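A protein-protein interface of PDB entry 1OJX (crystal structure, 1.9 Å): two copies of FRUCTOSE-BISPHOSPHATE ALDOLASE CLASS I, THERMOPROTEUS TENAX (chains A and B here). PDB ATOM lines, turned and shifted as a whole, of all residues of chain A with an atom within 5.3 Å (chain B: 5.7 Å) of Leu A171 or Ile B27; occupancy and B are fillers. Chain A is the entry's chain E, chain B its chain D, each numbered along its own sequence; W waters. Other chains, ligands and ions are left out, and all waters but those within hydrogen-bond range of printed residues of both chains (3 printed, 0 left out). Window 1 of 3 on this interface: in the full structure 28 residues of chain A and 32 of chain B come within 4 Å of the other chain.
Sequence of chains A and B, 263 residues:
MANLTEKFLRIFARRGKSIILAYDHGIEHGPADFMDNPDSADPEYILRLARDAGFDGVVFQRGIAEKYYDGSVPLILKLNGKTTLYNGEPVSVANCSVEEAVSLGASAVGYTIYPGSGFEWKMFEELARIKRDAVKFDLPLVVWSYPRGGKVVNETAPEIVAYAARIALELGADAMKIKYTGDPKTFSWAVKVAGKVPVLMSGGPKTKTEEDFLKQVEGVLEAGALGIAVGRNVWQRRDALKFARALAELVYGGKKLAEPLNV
OH of Tyr A163 lies within hydrogen-bond range of O of Ile B27, 2.8 Å away. The backbone carbonyl oxygen (O) of Glu B28 lies within hydrogen-bond range of the side-chain hydroxyl (OH) of Tyr A163. OH of Tyr A163 lies close to N of His B29 (3.5 Å). N of Gly B30 sits close to OH of Tyr A163 (3.4 Å). The backbone NH (N) of Gly B63 sits at hydrogen-bond distance from the backbone carbonyl oxygen (O) of Glu A170, at 2.9 Å. The backbone NH (N) of Thr B84 is in hydrogen-bond range of the side-chain hydroxyl (OH) of Tyr A163.
The backbone carbonyl oxygen of His B25 is in hydrogen-bond range of the backbone NH of Gly B30 (3.0 Å). OE2 of Glu B28 is in hydrogen-bond range of N of Lys B82 (3.1 Å). The backbone NH (N) of Thr B84 sits close to the backbone carbonyl oxygen (O) of Glu B28 (3.2 Å). The side-chain amide oxygen of Gln B61 lies within hydrogen-bond range of the side-chain amide nitrogen of Asn B95, 3.1 Å away. NH1 of Arg B62 sits at hydrogen-bond distance from O of Asn B95 (3.0 Å). NZ of Lys A131 is in hydrogen-bond range of O of Gly A172 (2.8 Å).
Phe A124 touches Gly B81 (CD2 to O, 3.9 Å). Arg B62 touches Lys A131. Gly B26 touches Tyr A163 (O to CE2, 3.6 Å). O of Gly B26 touches CG of Arg A166, 3.5 Å away. Thr B83 touches Ile A167 (CG2 to CD1, 3.7 Å). Gly B63 touches Leu A169 (CA to O, 3.3 Å). Gln B61 touches Glu A170 (CG to OE1, 3.4 Å). Glu A170 touches Arg B62 (O to CG, 3.9 Å). Leu A171 touches Ile B27 (CD2 to CD1, 3.7 Å). Leu A171 touches Arg B62.
Of chain B, only Ile B27 (3.7 Å), Arg B62 (3.6 Å) and Asn B95 (3.6 Å) come within 4 Å of Leu A171. Of chain A, only Tyr A163, Glu A170 and Leu A171 come within 4 Å of Ile B27. Of the printed residues of chain A, Thr B84 touches Tyr A163. Printed residues of chain A within 4 Å of Gly B63: Leu A169, Glu A170 and Gly A172. Of the printed residues of chain B, Glu A170 touches Gly B26, Ile B27, Gln B61, Arg B62 and Gly B63. Ala A173 touches none of the printed residues of chain B. Leu A127 touches none of the printed residues of chain B. The nearest residue of chain A that does not touch Ile B27 is Ile A167 (4.5 Å). The nearest printed residue of chain A that does not touch Gly B30 is Arg A166 (5.4 Å).
Hydrophobic or aromatic side chains of chain A that line the printed part of chain B: Phe A124, Tyr A163, Ile A167 and Leu A171. Hydrophobic or aromatic side chains of chain B that line the printed part of chain A: Ile B27. Among the printed residues, no Asp or Glu carboxylate lies within 4 Å of a Lys or Arg side-chain nitrogen of the other chain.
No position is printed for both chains.
Water W3 lies within hydrogen-bond range of OE2 of Glu A170, N of Gly B26 and NH2 of Arg A166. Water W2 lies within hydrogen-bond range of OE1 of Glu A170 (2.7 Å) and N of Gln B61 (2.9 Å). Water W1 lies within hydrogen-bond range of the backbone carbonyl oxygen of Leu A171 (2.9 Å) and the backbone carbonyl oxygen of Asn B95 (3.2 Å).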
ATOM      1  N   ILE A 113     -17.373  28.448  -5.519  1.00  0.00           N
ATOM      2  CA  ILE A 113     -16.619  27.266  -5.137  1.00  0.00           C
ATOM      3  C   ILE A 113     -16.590  27.135  -3.623  1.00  0.00           C
ATOM      4  O   ILE A 113     -16.638  28.153  -2.891  1.00  0.00           O
ATOM      5  CB  ILE A 113     -15.162  27.297  -5.705  1.00  0.00           C
ATOM      6  CG1 ILE A 113     -14.397  28.535  -5.237  1.00  0.00           C
ATOM      7  CG2 ILE A 113     -15.181  27.204  -7.239  1.00  0.00           C
ATOM      8  CD1 ILE A 113     -12.961  28.569  -5.703  1.00  0.00           C
ATOM      9  N   PHE A 124     -14.266  22.348  -9.231  1.00  0.00           N
ATOM     10  CA  PHE A 124     -13.051  22.734  -9.960  1.00  0.00           C
ATOM     11  C   PHE A 124     -13.107  22.276 -11.425  1.00  0.00           C
ATOM     12  O   PHE A 124     -12.708  23.012 -12.327  1.00  0.00           O
ATOM     13  CB  PHE A 124     -11.779  22.205  -9.275  1.00  0.00           C
ATOM     14  CG  PHE A 124     -11.488  22.832  -7.921  1.00  0.00           C
ATOM     15  CD1 PHE A 124     -12.214  23.922  -7.435  1.00  0.00           C
ATOM     16  CD2 PHE A 124     -10.464  22.337  -7.142  1.00  0.00           C
ATOM     17  CE1 PHE A 124     -11.930  24.474  -6.206  1.00  0.00           C
ATOM     18  CE2 PHE A 124     -10.166  22.903  -5.900  1.00  0.00           C
ATOM     19  CZ  PHE A 124     -10.896  23.968  -5.439  1.00  0.00           C
ATOM     20  N   LEU A 127     -15.755  24.556 -13.164  1.00  0.00           N
ATOM     21  CA  LEU A 127     -15.226  25.916 -13.281  1.00  0.00           C
ATOM     22  C   LEU A 127     -14.216  26.015 -14.431  1.00  0.00           C
ATOM     23  O   LEU A 127     -14.150  27.041 -15.098  1.00  0.00           O
ATOM     24  CB  LEU A 127     -14.578  26.380 -11.975  1.00  0.00           C
ATOM     25  CG  LEU A 127     -14.007  27.808 -11.954  1.00  0.00           C
ATOM     26  CD1 LEU A 127     -15.111  28.817 -12.285  1.00  0.00           C
ATOM     27  CD2 LEU A 127     -13.322  28.156 -10.644  1.00  0.00           C
ATOM     28  N   LYS A 131     -14.612  28.878 -17.108  1.00  0.00           N
ATOM     29  CA  LYS A 131     -13.503  29.791 -17.370  1.00  0.00           C
ATOM     30  C   LYS A 131     -13.129  29.853 -18.861  1.00  0.00           C
ATOM     31  O   LYS A 131     -12.924  30.928 -19.428  1.00  0.00           O
ATOM     32  CB  LYS A 131     -12.282  29.333 -16.559  1.00  0.00           C
ATOM     33  CG  LYS A 131     -10.974  30.098 -16.805  1.00  0.00           C
ATOM     34  CD  LYS A 131     -11.060  31.592 -16.476  1.00  0.00           C
ATOM     35  CE  LYS A 131      -9.745  32.309 -16.864  1.00  0.00           C
ATOM     36  NZ  LYS A 131      -9.741  33.789 -16.574  1.00  0.00           N
ATOM     37  N   TYR A 163      -6.914  32.093   2.313  1.00  0.00           N
ATOM     38  CA  TYR A 163      -6.878  30.901   1.447  1.00  0.00           C
ATOM     39  C   TYR A 163      -7.940  31.020   0.375  1.00  0.00           C
ATOM     40  O   TYR A 163      -7.672  30.744  -0.788  1.00  0.00           O
ATOM     41  CB  TYR A 163      -7.059  29.608   2.262  1.00  0.00           C
ATOM     42  CG  TYR A 163      -6.401  28.336   1.720  1.00  0.00           C
ATOM     43  CD1 TYR A 163      -6.134  27.258   2.580  1.00  0.00           C
ATOM     44  CD2 TYR A 163      -6.062  28.183   0.369  1.00  0.00           C
ATOM     45  CE1 TYR A 163      -5.535  26.073   2.109  1.00  0.00           C
ATOM     46  CE2 TYR A 163      -5.460  27.008  -0.115  1.00  0.00           C
ATOM     47  CZ  TYR A 163      -5.202  25.948   0.757  1.00  0.00           C
ATOM     48  OH  TYR A 163      -4.609  24.777   0.280  1.00  0.00           O
ATOM     49  N   ARG A 166      -6.667  33.497  -2.354  1.00  0.00           N
ATOM     50  CA  ARG A 166      -5.595  32.962  -3.189  1.00  0.00           C
ATOM     51  C   ARG A 166      -6.087  31.876  -4.173  1.00  0.00           C
ATOM     52  O   ARG A 166      -5.694  31.897  -5.347  1.00  0.00           O
ATOM     53  CB  ARG A 166      -4.414  32.470  -2.334  1.00  0.00           C
ATOM     54  CG  ARG A 166      -3.187  32.060  -3.118  1.00  0.00           C
ATOM     55  CD  ARG A 166      -2.743  33.096  -4.137  1.00  0.00           C
ATOM     56  NE  ARG A 166      -1.419  32.795  -4.656  1.00  0.00           N
ATOM     57  CZ  ARG A 166      -0.406  33.637  -4.706  1.00  0.00           C
ATOM     58  NH1 ARG A 166      -0.507  34.891  -4.269  1.00  0.00           N
ATOM     59  NH2 ARG A 166       0.745  33.213  -5.207  1.00  0.00           N
ATOM     60  N   ILE A 167      -6.969  30.969  -3.732  1.00  0.00           N
ATOM     61  CA  ILE A 167      -7.511  29.941  -4.636  1.00  0.00           C
ATOM     62  C   ILE A 167      -8.221  30.568  -5.840  1.00  0.00           C
ATOM     63  O   ILE A 167      -8.058  30.120  -6.988  1.00  0.00           O
ATOM     64  CB  ILE A 167      -8.473  28.985  -3.880  1.00  0.00           C
ATOM     65  CG1 ILE A 167      -7.707  28.155  -2.845  1.00  0.00           C
ATOM     66  CG2 ILE A 167      -9.183  28.047  -4.857  1.00  0.00           C
ATOM     67  CD1 ILE A 167      -8.608  27.529  -1.762  1.00  0.00           C
ATOM     68  N   ALA A 168      -9.016  31.604  -5.578  1.00  0.00           N
ATOM     69  CA  ALA A 168      -9.744  32.282  -6.637  1.00  0.00           C
ATOM     70  C   ALA A 168      -8.781  32.866  -7.689  1.00  0.00           C
ATOM     71  O   ALA A 168      -9.001  32.710  -8.892  1.00  0.00           O
ATOM     72  CB  ALA A 168     -10.664  33.344  -6.048  1.00  0.00           C
ATOM     73  N   LEU A 169      -7.696  33.493  -7.244  1.00  0.00           N
ATOM     74  CA  LEU A 169      -6.643  33.964  -8.165  1.00  0.00           C
ATOM     75  C   LEU A 169      -6.031  32.819  -8.983  1.00  0.00           C
ATOM     76  O   LEU A 169      -5.921  32.917 -10.214  1.00  0.00           O
ATOM     77  CB  LEU A 169      -5.523  34.695  -7.400  1.00  0.00           C
ATOM     78  CG  LEU A 169      -4.197  35.022  -8.127  1.00  0.00           C
ATOM     79  CD1 LEU A 169      -4.364  36.015  -9.298  1.00  0.00           C
ATOM     80  CD2 LEU A 169      -3.213  35.563  -7.145  1.00  0.00           C
ATOM     81  N   GLU A 170      -5.680  31.727  -8.301  1.00  0.00           N
ATOM     82  CA  GLU A 170      -4.992  30.585  -8.922  1.00  0.00           C
ATOM     83  C   GLU A 170      -5.842  29.913 -10.013  1.00  0.00           C
ATOM     84  O   GLU A 170      -5.313  29.439 -11.019  1.00  0.00           O
ATOM     85  CB  GLU A 170      -4.586  29.560  -7.847  1.00  0.00           C
ATOM     86  CG  GLU A 170      -3.622  30.094  -6.770  1.00  0.00           C
ATOM     87  CD  GLU A 170      -2.137  29.852  -7.049  1.00  0.00           C
ATOM     88  OE1 GLU A 170      -1.798  29.090  -7.972  1.00  0.00           O
ATOM     89  OE2 GLU A 170      -1.290  30.436  -6.326  1.00  0.00           O
ATOM     90  N   LEU A 171      -7.158  29.892  -9.820  1.00  0.00           N
ATOM     91  CA  LEU A 171      -8.067  29.157 -10.704  1.00  0.00           C
ATOM     92  C   LEU A 171      -8.544  30.001 -11.877  1.00  0.00           C
ATOM     93  O   LEU A 171      -9.202  29.488 -12.779  1.00  0.00           O
ATOM     94  CB  LEU A 171      -9.271  28.629  -9.913  1.00  0.00           C
ATOM     95  CG  LEU A 171      -8.965  27.496  -8.922  1.00  0.00           C
ATOM     96  CD1 LEU A 171     -10.214  27.084  -8.164  1.00  0.00           C
ATOM     97  CD2 LEU A 171      -8.350  26.283  -9.645  1.00  0.00           C
ATOM     98  N   GLY A 172      -8.254  31.295 -11.835  1.00  0.00           N
ATOM     99  CA  GLY A 172      -8.505  32.189 -12.963  1.00  0.00           C
ATOM    100  C   GLY A 172      -9.601  33.238 -12.824  1.00  0.00           C
ATOM    101  O   GLY A 172     -10.030  33.778 -13.824  1.00  0.00           O
ATOM    102  N   ALA A 173     -10.055  33.535 -11.609  1.00  0.00           N
ATOM    103  CA  ALA A 173     -11.022  34.622 -11.405  1.00  0.00           C
ATOM    104  C   ALA A 173     -10.497  35.953 -11.929  1.00  0.00           C
ATOM    105  O   ALA A 173      -9.302  36.260 -11.801  1.00  0.00           O
ATOM    106  CB  ALA A 173     -11.352  34.772  -9.966  1.00  0.00           C
ATOM    107  N   ASP B  24       3.169  26.383  -7.230  1.00  0.00           N
ATOM    108  CA  ASP B  24       1.761  25.990  -7.113  1.00  0.00           C
ATOM    109  C   ASP B  24       1.237  26.000  -5.669  1.00  0.00           C
ATOM    110  O   ASP B  24       0.088  25.657  -5.440  1.00  0.00           O
ATOM    111  CB  ASP B  24       1.492  24.639  -7.811  1.00  0.00           C
ATOM    112  CG  ASP B  24       2.240  23.471  -7.193  1.00  0.00           C
ATOM    113  OD1 ASP B  24       3.260  23.700  -6.507  1.00  0.00           O
ATOM    114  OD2 ASP B  24       1.898  22.274  -7.367  1.00  0.00           O
ATOM    115  N   HIS B  25       2.060  26.450  -4.720  1.00  0.00           N
ATOM    116  CA  HIS B  25       1.753  26.412  -3.276  1.00  0.00           C
ATOM    117  C   HIS B  25       0.449  27.133  -2.876  1.00  0.00           C
ATOM    118  O   HIS B  25      -0.243  26.723  -1.944  1.00  0.00           O
ATOM    119  CB  HIS B  25       2.948  27.015  -2.521  1.00  0.00           C
ATOM    120  CG  HIS B  25       2.926  26.848  -1.029  1.00  0.00           C
ATOM    121  ND1 HIS B  25       3.737  25.945  -0.370  1.00  0.00           N
ATOM    122  CD2 HIS B  25       2.280  27.540  -0.058  1.00  0.00           C
ATOM    123  CE1 HIS B  25       3.554  26.056   0.936  1.00  0.00           C
ATOM    124  NE2 HIS B  25       2.679  27.018   1.155  1.00  0.00           N
ATOM    125  N   GLY B  26       0.109  28.209  -3.577  1.00  0.00           N
ATOM    126  CA  GLY B  26      -1.010  29.044  -3.194  1.00  0.00           C
ATOM    127  C   GLY B  26      -2.344  28.302  -3.221  1.00  0.00           C
ATOM    128  O   GLY B  26      -3.226  28.594  -2.409  1.00  0.00           O
ATOM    129  N   ILE B  27      -2.507  27.374  -4.162  1.00  0.00           N
ATOM    130  CA  ILE B  27      -3.668  26.488  -4.158  1.00  0.00           C
ATOM    131  C   ILE B  27      -3.427  25.236  -3.293  1.00  0.00           C
ATOM    132  O   ILE B  27      -4.283  24.897  -2.481  1.00  0.00           O
ATOM    133  CB  ILE B  27      -4.191  26.126  -5.588  1.00  0.00           C
ATOM    134  CG1 ILE B  27      -5.496  25.307  -5.460  1.00  0.00           C
ATOM    135  CG2 ILE B  27      -3.187  25.305  -6.400  1.00  0.00           C
ATOM    136  CD1 ILE B  27      -6.264  25.101  -6.778  1.00  0.00           C
ATOM    137  N   GLU B  28      -2.255  24.604  -3.408  1.00  0.00           N
ATOM    138  CA  GLU B  28      -1.998  23.323  -2.724  1.00  0.00           C
ATOM    139  C   GLU B  28      -1.968  23.418  -1.190  1.00  0.00           C
ATOM    140  O   GLU B  28      -2.555  22.552  -0.511  1.00  0.00           O
ATOM    141  CB  GLU B  28      -0.699  22.682  -3.231  1.00  0.00           C
ATOM    142  CG  GLU B  28      -0.771  22.169  -4.665  1.00  0.00           C
ATOM    143  CD  GLU B  28      -1.682  20.945  -4.862  1.00  0.00           C
ATOM    144  OE1 GLU B  28      -1.833  20.123  -3.915  1.00  0.00           O
ATOM    145  OE2 GLU B  28      -2.249  20.791  -5.988  1.00  0.00           O
ATOM    146  N   HIS B  29      -1.297  24.455  -0.662  1.00  0.00           N
ATOM    147  CA  HIS B  29      -1.197  24.718   0.783  1.00  0.00           C
ATOM    148  C   HIS B  29      -1.777  26.054   1.284  1.00  0.00           C
ATOM    149  O   HIS B  29      -1.939  26.250   2.481  1.00  0.00           O
ATOM    150  CB  HIS B  29       0.278  24.614   1.209  1.00  0.00           C
ATOM    151  CG  HIS B  29       0.918  23.324   0.806  1.00  0.00           C
ATOM    152  ND1 HIS B  29       0.703  22.146   1.490  1.00  0.00           N
ATOM    153  CD2 HIS B  29       1.733  23.016  -0.230  1.00  0.00           C
ATOM    154  CE1 HIS B  29       1.371  21.170   0.899  1.00  0.00           C
ATOM    155  NE2 HIS B  29       2.001  21.670  -0.149  1.00  0.00           N
ATOM    156  N   GLY B  30      -2.070  26.986   0.389  1.00  0.00           N
ATOM    157  CA  GLY B  30      -2.591  28.278   0.799  1.00  0.00           C
ATOM    158  C   GLY B  30      -1.464  29.236   1.156  1.00  0.00           C
ATOM    159  O   GLY B  30      -0.305  28.823   1.259  1.00  0.00           O
ATOM    160  N   GLN B  61       0.073  27.573 -11.769  1.00  0.00           N
ATOM    161  CA  GLN B  61      -1.326  27.259 -12.123  1.00  0.00           C
ATOM    162  C   GLN B  61      -1.827  28.243 -13.184  1.00  0.00           C
ATOM    163  O   GLN B  61      -1.239  29.307 -13.354  1.00  0.00           O
ATOM    164  CB  GLN B  61      -2.198  27.368 -10.875  1.00  0.00           C
ATOM    165  CG  GLN B  61      -1.911  26.267  -9.839  1.00  0.00           C
ATOM    166  CD  GLN B  61      -2.639  24.953 -10.148  1.00  0.00           C
ATOM    167  OE1 GLN B  61      -3.656  24.952 -10.829  1.00  0.00           O
ATOM    168  NE2 GLN B  61      -2.110  23.849  -9.660  1.00  0.00           N
ATOM    169  N   ARG B  62      -2.928  27.911 -13.859  1.00  0.00           N
ATOM    170  CA  ARG B  62      -3.428  28.726 -14.978  1.00  0.00           C
ATOM    171  C   ARG B  62      -3.663  30.216 -14.622  1.00  0.00           C
ATOM    172  O   ARG B  62      -3.379  31.102 -15.433  1.00  0.00           O
ATOM    173  CB  ARG B  62      -4.711  28.101 -15.560  1.00  0.00           C
ATOM    174  CG  ARG B  62      -5.956  28.112 -14.607  1.00  0.00           C
ATOM    175  CD  ARG B  62      -7.282  27.823 -15.270  1.00  0.00           C
ATOM    176  NE  ARG B  62      -7.409  28.611 -16.492  1.00  0.00           N
ATOM    177  CZ  ARG B  62      -8.052  28.254 -17.590  1.00  0.00           C
ATOM    178  NH1 ARG B  62      -8.755  27.121 -17.669  1.00  0.00           N
ATOM    179  NH2 ARG B  62      -8.024  29.089 -18.618  1.00  0.00           N
ATOM    180  N   GLY B  63      -4.176  30.488 -13.419  1.00  0.00           N
ATOM    181  CA  GLY B  63      -4.560  31.847 -13.018  1.00  0.00           C
ATOM    182  C   GLY B  63      -3.385  32.788 -12.821  1.00  0.00           C
ATOM    183  O   GLY B  63      -3.418  33.976 -13.224  1.00  0.00           O
ATOM    184  N   GLY B  81      -4.955  20.791  -9.549  1.00  0.00           N
ATOM    185  CA  GLY B  81      -4.691  21.359  -8.235  1.00  0.00           C
ATOM    186  C   GLY B  81      -5.758  20.935  -7.249  1.00  0.00           C
ATOM    187  O   GLY B  81      -6.933  20.819  -7.628  1.00  0.00           O
ATOM    188  N   LYS B  82      -5.340  20.667  -6.006  1.00  0.00           N
ATOM    189  CA  LYS B  82      -6.259  20.473  -4.884  1.00  0.00           C
ATOM    190  C   LYS B  82      -5.823  21.309  -3.651  1.00  0.00           C
ATOM    191  O   LYS B  82      -4.768  21.918  -3.677  1.00  0.00           O
ATOM    192  CB  LYS B  82      -6.330  18.987  -4.534  1.00  0.00           C
ATOM    193  CG  LYS B  82      -5.069  18.399  -3.906  1.00  0.00           C
ATOM    194  CD  LYS B  82      -5.411  17.099  -3.158  1.00  0.00           C
ATOM    195  CE  LYS B  82      -4.611  16.899  -1.877  1.00  0.00           C
ATOM    196  NZ  LYS B  82      -4.732  17.893  -0.769  1.00  0.00           N
ATOM    197  N   THR B  83      -6.643  21.351  -2.593  1.00  0.00           N
ATOM    198  CA  THR B  83      -6.290  22.078  -1.364  1.00  0.00           C
ATOM    199  C   THR B  83      -6.010  21.130  -0.215  1.00  0.00           C
ATOM    200  O   THR B  83      -6.432  19.969  -0.226  1.00  0.00           O
ATOM    201  CB  THR B  83      -7.406  23.086  -0.925  1.00  0.00           C
ATOM    202  OG1 THR B  83      -8.548  22.383  -0.415  1.00  0.00           O
ATOM    203  CG2 THR B  83      -7.945  23.906  -2.102  1.00  0.00           C
ATOM    204  N   THR B  84      -5.319  21.627   0.806  1.00  0.00           N
ATOM    205  CA  THR B  84      -5.150  20.864   2.040  1.00  0.00           C
ATOM    206  C   THR B  84      -6.363  20.943   2.963  1.00  0.00           C
ATOM    207  O   THR B  84      -6.391  20.271   3.994  1.00  0.00           O
ATOM    208  CB  THR B  84      -3.916  21.320   2.853  1.00  0.00           C
ATOM    209  OG1 THR B  84      -4.009  22.719   3.142  1.00  0.00           O
ATOM    210  CG2 THR B  84      -2.668  21.178   2.056  1.00  0.00           C
ATOM    211  N   ASN B  95      -7.913  21.861 -13.930  1.00  0.00           N
ATOM    212  CA  ASN B  95      -8.672  23.114 -14.049  1.00  0.00           C
ATOM    213  C   ASN B  95      -8.332  23.875 -15.331  1.00  0.00           C
ATOM    214  O   ASN B  95      -8.755  25.013 -15.502  1.00  0.00           O
ATOM    215  CB  ASN B  95      -8.452  24.010 -12.829  1.00  0.00           C
ATOM    216  CG  ASN B  95      -7.002  24.354 -12.603  1.00  0.00           C
ATOM    217  OD1 ASN B  95      -6.391  25.077 -13.417  1.00  0.00           O
ATOM    218  ND2 ASN B  95      -6.437  23.876 -11.478  1.00  0.00           N
HETATM  219  O   HOH W   1     -10.424  27.110 -13.843  1.00  0.00           O
HETATM  220  O   HOH W   2       0.602  28.870  -9.240  1.00  0.00           O
HETATM  221  O   HOH W   3       1.191  30.096  -5.680  1.00  0.00           O
